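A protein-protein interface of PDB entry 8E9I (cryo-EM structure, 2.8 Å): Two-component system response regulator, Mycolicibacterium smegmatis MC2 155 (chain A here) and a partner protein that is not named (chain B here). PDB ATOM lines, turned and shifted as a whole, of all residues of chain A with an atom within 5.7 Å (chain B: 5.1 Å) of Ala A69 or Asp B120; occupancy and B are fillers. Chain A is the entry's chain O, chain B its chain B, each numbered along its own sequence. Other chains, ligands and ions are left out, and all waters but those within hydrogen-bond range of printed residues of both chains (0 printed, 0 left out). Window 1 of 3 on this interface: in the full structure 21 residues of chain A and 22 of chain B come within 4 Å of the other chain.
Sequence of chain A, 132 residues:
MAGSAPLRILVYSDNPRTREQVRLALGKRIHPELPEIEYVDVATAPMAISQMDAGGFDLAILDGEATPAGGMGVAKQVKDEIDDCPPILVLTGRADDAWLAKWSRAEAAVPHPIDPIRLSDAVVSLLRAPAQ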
ATOM      1  N   TYR A  12      30.099   4.313 -20.393  1.00  0.00           N
ATOM      2  CA  TYR A  12      28.669   4.067 -20.516  1.00  0.00           C
ATOM      3  C   TYR A  12      28.004   5.265 -21.172  1.00  0.00           C
ATOM      4  O   TYR A  12      28.116   6.391 -20.678  1.00  0.00           O
ATOM      5  CB  TYR A  12      28.032   3.805 -19.156  1.00  0.00           C
ATOM      6  CG  TYR A  12      26.526   3.747 -19.221  1.00  0.00           C
ATOM      7  CD1 TYR A  12      25.888   2.896 -20.107  1.00  0.00           C
ATOM      8  CD2 TYR A  12      25.743   4.557 -18.418  1.00  0.00           C
ATOM      9  CE1 TYR A  12      24.519   2.839 -20.179  1.00  0.00           C
ATOM     10  CE2 TYR A  12      24.370   4.510 -18.484  1.00  0.00           C
ATOM     11  CZ  TYR A  12      23.763   3.648 -19.366  1.00  0.00           C
ATOM     12  OH  TYR A  12      22.394   3.592 -19.442  1.00  0.00           O
ATOM     13  N   ALA A  45      21.900   0.447 -19.142  1.00  0.00           N
ATOM     14  CA  ALA A  45      22.146   0.402 -17.710  1.00  0.00           C
ATOM     15  C   ALA A  45      22.316  -1.033 -17.226  1.00  0.00           C
ATOM     16  O   ALA A  45      23.247  -1.305 -16.464  1.00  0.00           O
ATOM     17  CB  ALA A  45      21.020   1.093 -16.944  1.00  0.00           C
ATOM     18  N   ASP A  63      27.919   8.513 -18.879  1.00  0.00           N
ATOM     19  CA  ASP A  63      27.308   9.694 -19.475  1.00  0.00           C
ATOM     20  C   ASP A  63      26.094  10.089 -18.650  1.00  0.00           C
ATOM     21  O   ASP A  63      25.094   9.369 -18.621  1.00  0.00           O
ATOM     22  CB  ASP A  63      26.911   9.416 -20.919  1.00  0.00           C
ATOM     23  CG  ASP A  63      26.293  10.622 -21.601  1.00  0.00           C
ATOM     24  OD1 ASP A  63      26.364  11.734 -21.037  1.00  0.00           O
ATOM     25  OD2 ASP A  63      25.727  10.459 -22.701  1.00  0.00           O
ATOM     26  N   ALA A  66      22.666   9.757 -20.371  1.00  0.00           N
ATOM     27  CA  ALA A  66      22.186   8.505 -20.941  1.00  0.00           C
ATOM     28  C   ALA A  66      20.669   8.445 -20.883  1.00  0.00           C
ATOM     29  O   ALA A  66      20.068   8.717 -19.842  1.00  0.00           O
ATOM     30  CB  ALA A  66      22.797   7.321 -20.192  1.00  0.00           C
ATOM     31  N   THR A  67      20.053   8.077 -22.004  1.00  0.00           N
ATOM     32  CA  THR A  67      18.616   8.288 -22.164  1.00  0.00           C
ATOM     33  C   THR A  67      17.781   7.416 -21.244  1.00  0.00           C
ATOM     34  O   THR A  67      17.082   7.966 -20.378  1.00  0.00           O
ATOM     35  CB  THR A  67      18.225   8.062 -23.628  1.00  0.00           C
ATOM     36  N   PRO A  68      17.787   6.086 -21.364  1.00  0.00           N
ATOM     37  CA  PRO A  68      16.885   5.283 -20.528  1.00  0.00           C
ATOM     38  C   PRO A  68      17.298   5.211 -19.069  1.00  0.00           C
ATOM     39  O   PRO A  68      16.462   4.855 -18.231  1.00  0.00           O
ATOM     40  CB  PRO A  68      16.941   3.903 -21.191  1.00  0.00           C
ATOM     41  CG  PRO A  68      18.308   3.842 -21.760  1.00  0.00           C
ATOM     42  CD  PRO A  68      18.657   5.241 -22.195  1.00  0.00           C
ATOM     43  N   ALA A  69      18.553   5.523 -18.739  1.00  0.00           N
ATOM     44  CA  ALA A  69      18.994   5.533 -17.346  1.00  0.00           C
ATOM     45  C   ALA A  69      20.269   6.370 -17.273  1.00  0.00           C
ATOM     46  O   ALA A  69      21.311   5.954 -17.783  1.00  0.00           O
ATOM     47  CB  ALA A  69      19.222   4.124 -16.836  1.00  0.00           C
ATOM     48  N   GLY A  70      20.182   7.524 -16.621  1.00  0.00           N
ATOM     49  CA  GLY A  70      21.296   8.449 -16.619  1.00  0.00           C
ATOM     50  C   GLY A  70      22.513   7.883 -15.914  1.00  0.00           C
ATOM     51  O   GLY A  70      22.416   7.042 -15.024  1.00  0.00           O
ATOM     52  N   GLY A  71      23.683   8.368 -16.324  1.00  0.00           N
ATOM     53  CA  GLY A  71      24.921   7.926 -15.715  1.00  0.00           C
ATOM     54  C   GLY A  71      25.076   8.342 -14.268  1.00  0.00           C
ATOM     55  O   GLY A  71      25.846   7.719 -13.537  1.00  0.00           O
ATOM     56  N   VAL A  74      23.145   5.631 -12.431  1.00  0.00           N
ATOM     57  CA  VAL A  74      23.970   4.433 -12.442  1.00  0.00           C
ATOM     58  C   VAL A  74      25.154   4.600 -11.505  1.00  0.00           C
ATOM     59  O   VAL A  74      25.594   3.641 -10.873  1.00  0.00           O
ATOM     60  CB  VAL A  74      24.431   4.104 -13.871  1.00  0.00           C
ATOM     61  CG1 VAL A  74      25.336   2.893 -13.857  1.00  0.00           C
ATOM     62  CG2 VAL A  74      23.243   3.860 -14.770  1.00  0.00           C
ATOM     63  N   ALA B 104       8.153  14.532 -15.842  1.00  0.00           N
ATOM     64  CA  ALA B 104       8.896  13.368 -15.388  1.00  0.00           C
ATOM     65  C   ALA B 104       9.724  12.768 -16.512  1.00  0.00           C
ATOM     66  O   ALA B 104      10.873  12.366 -16.300  1.00  0.00           O
ATOM     67  CB  ALA B 104       7.936  12.325 -14.823  1.00  0.00           C
ATOM     68  N   GLY B 118      13.975  15.037 -16.680  1.00  0.00           N
ATOM     69  CA  GLY B 118      13.776  13.622 -16.901  1.00  0.00           C
ATOM     70  C   GLY B 118      14.311  12.782 -15.767  1.00  0.00           C
ATOM     71  O   GLY B 118      15.497  12.851 -15.442  1.00  0.00           O
ATOM     72  N   VAL B 119      13.446  11.975 -15.154  1.00  0.00           N
ATOM     73  CA  VAL B 119      13.901  11.099 -14.089  1.00  0.00           C
ATOM     74  C   VAL B 119      14.878  10.068 -14.616  1.00  0.00           C
ATOM     75  O   VAL B 119      15.616   9.464 -13.835  1.00  0.00           O
ATOM     76  CB  VAL B 119      12.714  10.407 -13.407  1.00  0.00           C
ATOM     77  CG1 VAL B 119      11.735  11.428 -12.965  1.00  0.00           C
ATOM     78  CG2 VAL B 119      12.062   9.420 -14.346  1.00  0.00           C
ATOM     79  N   ASP B 120      14.898   9.850 -15.930  1.00  0.00           N
ATOM     80  CA  ASP B 120      15.910   8.986 -16.518  1.00  0.00           C
ATOM     81  C   ASP B 120      17.296   9.346 -16.012  1.00  0.00           C
ATOM     82  O   ASP B 120      18.186   8.491 -15.970  1.00  0.00           O
ATOM     83  CB  ASP B 120      15.859   9.091 -18.039  1.00  0.00           C
ATOM     84  N   HIS B 121      17.497  10.603 -15.616  1.00  0.00           N
ATOM     85  CA  HIS B 121      18.785  11.016 -15.085  1.00  0.00           C
ATOM     86  C   HIS B 121      19.125  10.288 -13.795  1.00  0.00           C
ATOM     87  O   HIS B 121      20.305  10.100 -13.484  1.00  0.00           O
ATOM     88  CB  HIS B 121      18.786  12.522 -14.839  1.00  0.00           C
ATOM     89  CG  HIS B 121      18.926  13.333 -16.085  1.00  0.00           C
ATOM     90  ND1 HIS B 121      20.117  13.909 -16.468  1.00  0.00           N
ATOM     91  CD2 HIS B 121      18.024  13.665 -17.036  1.00  0.00           C
ATOM     92  CE1 HIS B 121      19.942  14.562 -17.602  1.00  0.00           C
ATOM     93  NE2 HIS B 121      18.681  14.428 -17.969  1.00  0.00           N
ATOM     94  N   VAL B 122      18.118   9.873 -13.030  1.00  0.00           N
ATOM     95  CA  VAL B 122      18.362   9.383 -11.680  1.00  0.00           C
ATOM     96  C   VAL B 122      17.895   7.944 -11.513  1.00  0.00           C
ATOM     97  O   VAL B 122      18.431   7.208 -10.678  1.00  0.00           O
ATOM     98  CB  VAL B 122      17.681  10.296 -10.650  1.00  0.00           C
ATOM     99  CG1 VAL B 122      18.263  11.689 -10.737  1.00  0.00           C
ATOM    100  CG2 VAL B 122      16.184  10.325 -10.868  1.00  0.00           C
ATOM    101  N   VAL B 123      16.895   7.528 -12.283  1.00  0.00           N
ATOM    102  CA  VAL B 123      16.374   6.169 -12.167  1.00  0.00           C
ATOM    103  C   VAL B 123      16.080   5.618 -13.555  1.00  0.00           C
ATOM    104  O   VAL B 123      15.670   6.377 -14.442  1.00  0.00           O
ATOM    105  CB  VAL B 123      15.113   6.126 -11.293  1.00  0.00           C
ATOM    106  CG1 VAL B 123      15.455   6.466  -9.867  1.00  0.00           C
ATOM    107  CG2 VAL B 123      14.058   7.074 -11.831  1.00  0.00           C
ATOM    108  N   PRO B 124      16.262   4.323 -13.791  1.00  0.00           N
ATOM    109  CA  PRO B 124      15.870   3.760 -15.086  1.00  0.00           C
ATOM    110  C   PRO B 124      14.373   3.905 -15.303  1.00  0.00           C
ATOM    111  O   PRO B 124      13.572   3.637 -14.410  1.00  0.00           O
ATOM    112  CB  PRO B 124      16.288   2.290 -14.978  1.00  0.00           C
ATOM    113  CG  PRO B 124      17.267   2.243 -13.871  1.00  0.00           C
ATOM    114  CD  PRO B 124      16.849   3.301 -12.913  1.00  0.00           C
ATOM    115  N   VAL B 125      14.000   4.310 -16.508  1.00  0.00           N
ATOM    116  CA  VAL B 125      12.603   4.508 -16.867  1.00  0.00           C
ATOM    117  C   VAL B 125      12.163   3.345 -17.740  1.00  0.00           C
ATOM    118  O   VAL B 125      12.822   3.016 -18.732  1.00  0.00           O
ATOM    119  CB  VAL B 125      12.394   5.848 -17.591  1.00  0.00           C
ATOM    120  CG1 VAL B 125      10.967   5.961 -18.072  1.00  0.00           C
ATOM    121  CG2 VAL B 125      12.739   6.997 -16.673  1.00  0.00           C
ATOM    122  N   TYR B 128       7.788   5.902 -20.949  1.00  0.00           N
ATOM    123  CA  TYR B 128       7.596   7.343 -20.939  1.00  0.00           C
ATOM    124  C   TYR B 128       6.162   7.647 -21.333  1.00  0.00           C
ATOM    125  O   TYR B 128       5.609   6.995 -22.222  1.00  0.00           O
ATOM    126  CB  TYR B 128       8.555   8.030 -21.905  1.00  0.00           C
ATOM    127  CG  TYR B 128      10.003   7.891 -21.535  1.00  0.00           C
ATOM    128  CD1 TYR B 128      10.604   8.791 -20.675  1.00  0.00           C
ATOM    129  CD2 TYR B 128      10.768   6.861 -22.040  1.00  0.00           C
ATOM    130  CE1 TYR B 128      11.925   8.674 -20.337  1.00  0.00           C
ATOM    131  CE2 TYR B 128      12.093   6.735 -21.705  1.00  0.00           C
ATOM    132  CZ  TYR B 128      12.666   7.645 -20.855  1.00  0.00           C
ATOM    133  OH  TYR B 128      13.991   7.523 -20.514  1.00  0.00           O
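The side-chain hydroxyl (OH) of Tyr B128 is in hydrogen-bond range of the backbone carbonyl oxygen (O) of Thr A67, at 3.1 Å.
N of Val B125 sits at hydrogen-bond distance from O of Pro A68 (3.1 Å).
N of Gly A70 lies close to O of Asp B120, at 2.3 Å.
The side-chain hydroxyl (OH) of Tyr A12 lies within hydrogen-bond range of the backbone carbonyl oxygen (O) of Ala A69 (3.1 Å).
Thr A67 touches Asp B120 (O to CB, 2.9 Å).
Pro B124 touches Pro A68 (CA to O, 3.4 Å).
CA of Pro A68 touches OH of Tyr B128, at 3.7 Å.
C of Ala A69 touches O of Asp B120, at 3.2 Å.
CB of Ala A69 touches CA of Pro B124 (3.8 Å).
Gly A70 touches His B121.
Asp B120 touches just these residues of chain A: Thr A67 (2.9 Å), Ala A69 (3.2 Å) and Gly A70 (2.3 Å).
Of the printed residues of chain A, Val B125 touches Pro A68.
Of the printed residues of chain A, Pro B124 touches Pro A68 and Ala A69.
Of the printed residues of chain B, Pro A68 touches Pro B124 (3.4 Å), Val B125 (3.1 Å) and Tyr B128 (3.7 Å).
Printed residues of chain B within 4 Å of Gly A70: Asp B120 and His B121.
Val B122 touches none of the printed residues of chain A.
The nearest residue of chain B that does not touch Ala A69 is Val B123 (4.5 Å).
The nearest residue of chain A that does not touch Asp B120 is Pro A68 (4.3 Å).
The nearest printed residue of chain A that does not touch Pro B124 is Ala A45 (5.0 Å).
Hydrophobic or aromatic side chains of chain B that line the printed part of chain A: Pro B124 and Tyr B128.
Along chain B the printed residues that touch a printed residue of chain A span positions 120 to 128.
Among the printed residues, 9 pairs touch across the chains.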
